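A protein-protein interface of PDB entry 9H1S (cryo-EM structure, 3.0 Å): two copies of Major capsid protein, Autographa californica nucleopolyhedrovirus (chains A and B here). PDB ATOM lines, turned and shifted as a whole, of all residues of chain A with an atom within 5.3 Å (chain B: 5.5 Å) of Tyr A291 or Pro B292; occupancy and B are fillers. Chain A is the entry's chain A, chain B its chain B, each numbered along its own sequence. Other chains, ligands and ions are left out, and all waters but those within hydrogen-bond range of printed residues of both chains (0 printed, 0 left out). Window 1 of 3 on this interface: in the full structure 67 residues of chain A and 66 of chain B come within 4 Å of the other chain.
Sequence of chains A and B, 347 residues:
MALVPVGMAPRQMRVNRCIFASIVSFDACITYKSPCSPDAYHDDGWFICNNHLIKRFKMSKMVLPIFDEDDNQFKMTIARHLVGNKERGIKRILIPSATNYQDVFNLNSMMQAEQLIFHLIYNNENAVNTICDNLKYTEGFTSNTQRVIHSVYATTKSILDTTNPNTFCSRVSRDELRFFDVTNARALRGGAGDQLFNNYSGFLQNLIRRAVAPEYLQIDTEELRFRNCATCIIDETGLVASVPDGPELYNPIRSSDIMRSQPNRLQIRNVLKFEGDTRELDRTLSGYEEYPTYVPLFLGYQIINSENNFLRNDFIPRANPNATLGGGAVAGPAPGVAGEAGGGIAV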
ATOM      1  N   PRO A  65      -6.262   8.106  32.692  1.00  0.00           N
ATOM      2  CA  PRO A  65      -6.260   6.818  33.350  1.00  0.00           C
ATOM      3  C   PRO A  65      -4.886   6.503  33.867  1.00  0.00           C
ATOM      4  O   PRO A  65      -4.010   6.109  33.103  1.00  0.00           O
ATOM      5  CB  PRO A  65      -6.679   5.849  32.258  1.00  0.00           C
ATOM      6  CG  PRO A  65      -6.190   6.471  31.006  1.00  0.00           C
ATOM      7  CD  PRO A  65      -6.291   7.948  31.235  1.00  0.00           C
ATOM      8  N   ARG A 227       4.462  14.571  33.788  1.00  0.00           N
ATOM      9  CA  ARG A 227       5.007  15.311  32.684  1.00  0.00           C
ATOM     10  C   ARG A 227       6.104  16.187  33.186  1.00  0.00           C
ATOM     11  O   ARG A 227       6.034  16.725  34.287  1.00  0.00           O
ATOM     12  CB  ARG A 227       3.948  16.129  31.993  1.00  0.00           C
ATOM     13  CG  ARG A 227       4.388  16.801  30.701  1.00  0.00           C
ATOM     14  CD  ARG A 227       3.246  17.503  30.096  1.00  0.00           C
ATOM     15  NE  ARG A 227       2.225  16.568  29.685  1.00  0.00           N
ATOM     16  CZ  ARG A 227       2.045  16.088  28.443  1.00  0.00           C
ATOM     17  NH1 ARG A 227       2.797  16.510  27.455  1.00  0.00           N
ATOM     18  NH2 ARG A 227       1.089  15.197  28.236  1.00  0.00           N
ATOM     19  N   GLU A 289      -0.502   1.504  16.777  1.00  0.00           N
ATOM     20  CA  GLU A 289      -1.240   2.254  17.789  1.00  0.00           C
ATOM     21  C   GLU A 289      -0.893   3.722  17.721  1.00  0.00           C
ATOM     22  O   GLU A 289       0.279   4.082  17.651  1.00  0.00           O
ATOM     23  CB  GLU A 289      -0.939   1.733  19.188  1.00  0.00           C
ATOM     24  CG  GLU A 289      -1.761   2.395  20.287  1.00  0.00           C
ATOM     25  CD  GLU A 289      -1.467   1.839  21.655  1.00  0.00           C
ATOM     26  OE1 GLU A 289      -0.659   0.947  21.746  1.00  0.00           O
ATOM     27  OE2 GLU A 289      -2.050   2.302  22.610  1.00  0.00           O
ATOM     28  N   GLU A 290      -1.911   4.562  17.743  1.00  0.00           N
ATOM     29  CA  GLU A 290      -1.702   5.989  17.644  1.00  0.00           C
ATOM     30  C   GLU A 290      -1.615   6.684  18.986  1.00  0.00           C
ATOM     31  O   GLU A 290      -2.295   6.320  19.944  1.00  0.00           O
ATOM     32  CB  GLU A 290      -2.829   6.616  16.844  1.00  0.00           C
ATOM     33  CG  GLU A 290      -2.898   6.157  15.401  1.00  0.00           C
ATOM     34  CD  GLU A 290      -4.068   6.745  14.668  1.00  0.00           C
ATOM     35  OE1 GLU A 290      -4.790   7.507  15.263  1.00  0.00           O
ATOM     36  OE2 GLU A 290      -4.256   6.417  13.519  1.00  0.00           O
ATOM     37  N   TYR A 291      -0.798   7.716  19.021  1.00  0.00           N
ATOM     38  CA  TYR A 291      -0.639   8.581  20.168  1.00  0.00           C
ATOM     39  C   TYR A 291      -1.190   9.927  19.746  1.00  0.00           C
ATOM     40  O   TYR A 291      -0.736  10.470  18.745  1.00  0.00           O
ATOM     41  CB  TYR A 291       0.822   8.711  20.563  1.00  0.00           C
ATOM     42  CG  TYR A 291       1.061   9.609  21.744  1.00  0.00           C
ATOM     43  CD1 TYR A 291       0.932   9.120  23.032  1.00  0.00           C
ATOM     44  CD2 TYR A 291       1.402  10.928  21.539  1.00  0.00           C
ATOM     45  CE1 TYR A 291       1.153   9.953  24.111  1.00  0.00           C
ATOM     46  CE2 TYR A 291       1.624  11.761  22.610  1.00  0.00           C
ATOM     47  CZ  TYR A 291       1.505  11.279  23.894  1.00  0.00           C
ATOM     48  OH  TYR A 291       1.746  12.115  24.963  1.00  0.00           O
ATOM     49  N   PRO A 292      -2.133  10.499  20.481  1.00  0.00           N
ATOM     50  CA  PRO A 292      -2.849  11.716  20.169  1.00  0.00           C
ATOM     51  C   PRO A 292      -1.957  12.927  20.223  1.00  0.00           C
ATOM     52  O   PRO A 292      -0.985  12.978  20.972  1.00  0.00           O
ATOM     53  CB  PRO A 292      -3.916  11.790  21.249  1.00  0.00           C
ATOM     54  CG  PRO A 292      -3.350  11.026  22.390  1.00  0.00           C
ATOM     55  CD  PRO A 292      -2.565   9.920  21.758  1.00  0.00           C
ATOM     56  N   THR A 293      -2.323  13.921  19.431  1.00  0.00           N
ATOM     57  CA  THR A 293      -1.573  15.157  19.326  1.00  0.00           C
ATOM     58  C   THR A 293      -2.259  16.281  20.087  1.00  0.00           C
ATOM     59  O   THR A 293      -2.079  17.455  19.767  1.00  0.00           O
ATOM     60  CB  THR A 293      -1.406  15.564  17.855  1.00  0.00           C
ATOM     61  OG1 THR A 293      -2.700  15.728  17.263  1.00  0.00           O
ATOM     62  CG2 THR A 293      -0.638  14.490  17.087  1.00  0.00           C
ATOM     63  N   MET B  62       4.601   3.180  17.675  1.00  0.00           N
ATOM     64  CA  MET B  62       3.396   3.993  17.641  1.00  0.00           C
ATOM     65  C   MET B  62       3.387   5.004  16.493  1.00  0.00           C
ATOM     66  O   MET B  62       4.358   5.147  15.751  1.00  0.00           O
ATOM     67  CB  MET B  62       3.200   4.725  18.955  1.00  0.00           C
ATOM     68  CG  MET B  62       3.074   3.835  20.167  1.00  0.00           C
ATOM     69  SD  MET B  62       2.622   4.776  21.614  1.00  0.00           S
ATOM     70  CE  MET B  62       0.912   5.024  21.172  1.00  0.00           C
ATOM     71  N   VAL B  63       2.257   5.683  16.347  1.00  0.00           N
ATOM     72  CA  VAL B  63       2.046   6.695  15.318  1.00  0.00           C
ATOM     73  C   VAL B  63       1.516   8.031  15.807  1.00  0.00           C
ATOM     74  O   VAL B  63       0.662   8.086  16.682  1.00  0.00           O
ATOM     75  CB  VAL B  63       1.090   6.164  14.258  1.00  0.00           C
ATOM     76  CG1 VAL B  63       0.712   7.257  13.295  1.00  0.00           C
ATOM     77  CG2 VAL B  63       1.783   5.073  13.484  1.00  0.00           C
ATOM     78  N   LEU B  64       2.031   9.113  15.237  1.00  0.00           N
ATOM     79  CA  LEU B  64       1.541  10.450  15.502  1.00  0.00           C
ATOM     80  C   LEU B  64       0.699  10.926  14.330  1.00  0.00           C
ATOM     81  O   LEU B  64       1.252  11.435  13.358  1.00  0.00           O
ATOM     82  CB  LEU B  64       2.672  11.452  15.666  1.00  0.00           C
ATOM     83  CG  LEU B  64       3.662  11.187  16.775  1.00  0.00           C
ATOM     84  CD1 LEU B  64       4.740  12.256  16.727  1.00  0.00           C
ATOM     85  CD2 LEU B  64       2.931  11.199  18.099  1.00  0.00           C
ATOM     86  N   PRO B  65      -0.620  10.772  14.373  1.00  0.00           N
ATOM     87  CA  PRO B  65      -1.577  11.184  13.379  1.00  0.00           C
ATOM     88  C   PRO B  65      -1.669  12.685  13.415  1.00  0.00           C
ATOM     89  O   PRO B  65      -2.553  13.241  14.057  1.00  0.00           O
ATOM     90  CB  PRO B  65      -2.865  10.515  13.819  1.00  0.00           C
ATOM     91  CG  PRO B  65      -2.747  10.462  15.296  1.00  0.00           C
ATOM     92  CD  PRO B  65      -1.292  10.206  15.550  1.00  0.00           C
ATOM     93  N   ILE B  78       6.652   6.930  15.657  1.00  0.00           N
ATOM     94  CA  ILE B  78       7.248   7.272  16.937  1.00  0.00           C
ATOM     95  C   ILE B  78       7.247   6.071  17.860  1.00  0.00           C
ATOM     96  O   ILE B  78       6.325   5.270  17.831  1.00  0.00           O
ATOM     97  CB  ILE B  78       6.495   8.406  17.620  1.00  0.00           C
ATOM     98  CG1 ILE B  78       7.287   8.882  18.835  1.00  0.00           C
ATOM     99  CG2 ILE B  78       5.122   7.925  18.036  1.00  0.00           C
ATOM    100  CD1 ILE B  78       6.786  10.169  19.410  1.00  0.00           C
ATOM    101  N   ARG B 227       6.065  19.178  21.120  1.00  0.00           N
ATOM    102  CA  ARG B 227       6.237  19.031  22.548  1.00  0.00           C
ATOM    103  C   ARG B 227       7.238  20.035  23.006  1.00  0.00           C
ATOM    104  O   ARG B 227       8.262  20.233  22.362  1.00  0.00           O
ATOM    105  CB  ARG B 227       6.667  17.636  22.910  1.00  0.00           C
ATOM    106  CG  ARG B 227       6.712  17.354  24.397  1.00  0.00           C
ATOM    107  CD  ARG B 227       7.088  15.950  24.633  1.00  0.00           C
ATOM    108  NE  ARG B 227       6.069  15.054  24.132  1.00  0.00           N
ATOM    109  CZ  ARG B 227       5.074  14.505  24.852  1.00  0.00           C
ATOM    110  NH1 ARG B 227       4.997  14.723  26.143  1.00  0.00           N
ATOM    111  NH2 ARG B 227       4.187  13.736  24.240  1.00  0.00           N
ATOM    112  N   GLU B 290     -10.320   9.192  26.629  1.00  0.00           N
ATOM    113  CA  GLU B 290      -9.115   9.101  27.428  1.00  0.00           C
ATOM    114  C   GLU B 290      -7.853   9.504  26.691  1.00  0.00           C
ATOM    115  O   GLU B 290      -7.700   9.260  25.495  1.00  0.00           O
ATOM    116  CB  GLU B 290      -8.942   7.681  27.942  1.00  0.00           C
ATOM    117  CG  GLU B 290     -10.038   7.229  28.884  1.00  0.00           C
ATOM    118  CD  GLU B 290      -9.871   5.808  29.333  1.00  0.00           C
ATOM    119  OE1 GLU B 290      -8.909   5.190  28.945  1.00  0.00           O
ATOM    120  OE2 GLU B 290     -10.718   5.330  30.052  1.00  0.00           O
ATOM    121  N   TYR B 291      -6.942  10.093  27.440  1.00  0.00           N
ATOM    122  CA  TYR B 291      -5.628  10.482  26.976  1.00  0.00           C
ATOM    123  C   TYR B 291      -4.645   9.554  27.661  1.00  0.00           C
ATOM    124  O   TYR B 291      -4.673   9.454  28.882  1.00  0.00           O
ATOM    125  CB  TYR B 291      -5.342  11.934  27.335  1.00  0.00           C
ATOM    126  CG  TYR B 291      -3.965  12.415  26.969  1.00  0.00           C
ATOM    127  CD1 TYR B 291      -3.697  12.873  25.692  1.00  0.00           C
ATOM    128  CD2 TYR B 291      -2.964  12.392  27.919  1.00  0.00           C
ATOM    129  CE1 TYR B 291      -2.428  13.307  25.366  1.00  0.00           C
ATOM    130  CE2 TYR B 291      -1.696  12.823  27.596  1.00  0.00           C
ATOM    131  CZ  TYR B 291      -1.424  13.280  26.325  1.00  0.00           C
ATOM    132  OH  TYR B 291      -0.157  13.718  26.006  1.00  0.00           O
ATOM    133  N   PRO B 292      -3.759   8.889  26.927  1.00  0.00           N
ATOM    134  CA  PRO B 292      -2.819   7.888  27.392  1.00  0.00           C
ATOM    135  C   PRO B 292      -1.737   8.470  28.260  1.00  0.00           C
ATOM    136  O   PRO B 292      -1.383   9.641  28.147  1.00  0.00           O
ATOM    137  CB  PRO B 292      -2.227   7.334  26.106  1.00  0.00           C
ATOM    138  CG  PRO B 292      -2.351   8.443  25.128  1.00  0.00           C
ATOM    139  CD  PRO B 292      -3.643   9.117  25.484  1.00  0.00           C
ATOM    140  N   THR B 293      -1.184   7.619  29.111  1.00  0.00           N
ATOM    141  CA  THR B 293      -0.130   8.001  30.033  1.00  0.00           C
ATOM    142  C   THR B 293       1.195   7.442  29.566  1.00  0.00           C
ATOM    143  O   THR B 293       2.052   7.079  30.372  1.00  0.00           O
ATOM    144  CB  THR B 293      -0.425   7.490  31.446  1.00  0.00           C
ATOM    145  OG1 THR B 293      -0.559   6.063  31.417  1.00  0.00           O
ATOM    146  CG2 THR B 293      -1.716   8.099  31.960  1.00  0.00           C
ATOM    147  N   TYR B 294       1.340   7.353  28.257  1.00  0.00           N
ATOM    148  CA  TYR B 294       2.522   6.837  27.622  1.00  0.00           C
ATOM    149  C   TYR B 294       3.618   7.853  27.650  1.00  0.00           C
ATOM    150  O   TYR B 294       3.361   9.043  27.829  1.00  0.00           O
ATOM    151  CB  TYR B 294       2.228   6.506  26.184  1.00  0.00           C
ATOM    152  CG  TYR B 294       1.248   5.395  25.994  1.00  0.00           C
ATOM    153  CD1 TYR B 294       1.049   4.442  26.974  1.00  0.00           C
ATOM    154  CD2 TYR B 294       0.561   5.325  24.807  1.00  0.00           C
ATOM    155  CE1 TYR B 294       0.154   3.415  26.748  1.00  0.00           C
ATOM    156  CE2 TYR B 294      -0.328   4.307  24.581  1.00  0.00           C
ATOM    157  CZ  TYR B 294      -0.535   3.350  25.540  1.00  0.00           C
ATOM    158  OH  TYR B 294      -1.425   2.327  25.297  1.00  0.00           O
ATOM    159  N   PRO B 296       6.272   8.755  24.940  1.00  0.00           N
ATOM    160  CA  PRO B 296       6.830   8.735  23.603  1.00  0.00           C
ATOM    161  C   PRO B 296       8.209   9.344  23.577  1.00  0.00           C
ATOM    162  O   PRO B 296       8.538  10.181  24.418  1.00  0.00           O
ATOM    163  CB  PRO B 296       5.880   9.579  22.784  1.00  0.00           C
ATOM    164  CG  PRO B 296       4.639   9.644  23.568  1.00  0.00           C
ATOM    165  CD  PRO B 296       5.098   9.638  24.986  1.00  0.00           C
ATOM    166  N   PHE B 298      10.781  11.852  22.296  1.00  0.00           N
ATOM    167  CA  PHE B 298      10.986  13.160  21.676  1.00  0.00           C
ATOM    168  C   PHE B 298      12.368  13.775  21.859  1.00  0.00           C
ATOM    169  O   PHE B 298      12.887  13.898  22.974  1.00  0.00           O
ATOM    170  CB  PHE B 298       9.963  14.171  22.156  1.00  0.00           C
ATOM    171  CG  PHE B 298       8.612  14.012  21.546  1.00  0.00           C
ATOM    172  CD1 PHE B 298       7.687  13.091  21.997  1.00  0.00           C
ATOM    173  CD2 PHE B 298       8.264  14.843  20.499  1.00  0.00           C
ATOM    174  CE1 PHE B 298       6.441  13.011  21.397  1.00  0.00           C
ATOM    175  CE2 PHE B 298       7.029  14.763  19.905  1.00  0.00           C
ATOM    176  CZ  PHE B 298       6.114  13.843  20.355  1.00  0.00           C
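N of Met B62 sits at hydrogen-bond distance from O of Ile B78 (2.7 Å).
Pro A65 touches Glu B290, and with the chains exchanged Glu A290 touches Pro B65. Arg A227 touches Tyr B291, and with the chains exchanged Tyr A291 touches Arg B227. Tyr B291 touches its own counterpart, Tyr A291. Pro B292 touches its own counterpart, Pro A292. Of the 22 pairs that touch across the chains among the printed residues, 13 have their exchanged pair printed and touching as well.
The guanidinium group (NH2) of Arg A227 is in hydrogen-bond range of the side-chain hydroxyl (OH) of Tyr B291 (3.0 Å). The side-chain hydroxyl of Tyr A291 sits at hydrogen-bond distance from the side-chain hydroxyl of Tyr B291. N of Val B63 lies within hydrogen-bond range of O of Glu A289, 2.9 Å away. The side-chain hydroxyl (OH) of Tyr B294 is in hydrogen-bond range of the side-chain carboxylate (OE2) of Glu A289 (2.8 Å). NH2 of Arg B227 sits at hydrogen-bond distance from OH of Tyr A291, at 3.0 Å. The guanidinium group of Arg B227 lies close to the guanidinium group of Arg A227 (3.1 Å). The backbone carbonyl oxygen (O) of Val B63 is in hydrogen-bond range of the backbone NH (N) of Tyr A291, 2.8 Å away.
Tyr A291 touches just these residues of chain B: Met B62 (3.7 Å), Val B63 (2.8 Å), Leu B64 (3.8 Å), Pro B65 (3.3 Å), Arg B227 (3.0 Å), Tyr B291 (2.7 Å), Pro B292 (3.9 Å) and Pro B296 (3.5 Å). Of the printed residues of chain A, Pro B65 touches Glu A290, Tyr A291 and Thr A293. Of the printed residues of chain A, Pro B292 touches Tyr A291 and Pro A292. Printed residues of chain A within 4 Å of Tyr B294: Glu A289 (2.8 Å). Phe B298 touches none of the printed residues of chain A. The nearest printed residue of chain A that does not touch Glu B290 is Pro A292 (5.6 Å).
Hydrophobic or aromatic side chains of chain B that line the printed part of chain A: Met B62, Leu B64, Pro B65, Tyr B291, Pro B292, Tyr B294 and Pro B296. Hydrophobic or aromatic side chains of chain A within 4 Å of the printed part of chain B: Pro A65, Tyr A291 and Pro A292. Among the printed residues, no Asp or Glu carboxylate lies within 4 Å of a Lys or Arg side-chain nitrogen of the other chain.
Glu B290 touches Pro A65. Pro A65 touches Tyr B291. Glu A289 touches Met B62 (O to CA, 3.1 Å). Met B62 touches Glu A290. CG of Pro B65 touches OE1 of Glu A290, 3.6 Å away. Tyr A291 touches Leu B64 (CD2 to CD2, 3.8 Å). CE1 of Tyr A291 touches CG of Pro B292, at 3.9 Å. Tyr B291 touches Pro A292. Pro B292 touches Pro A292. Pro B65 touches Thr A293.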
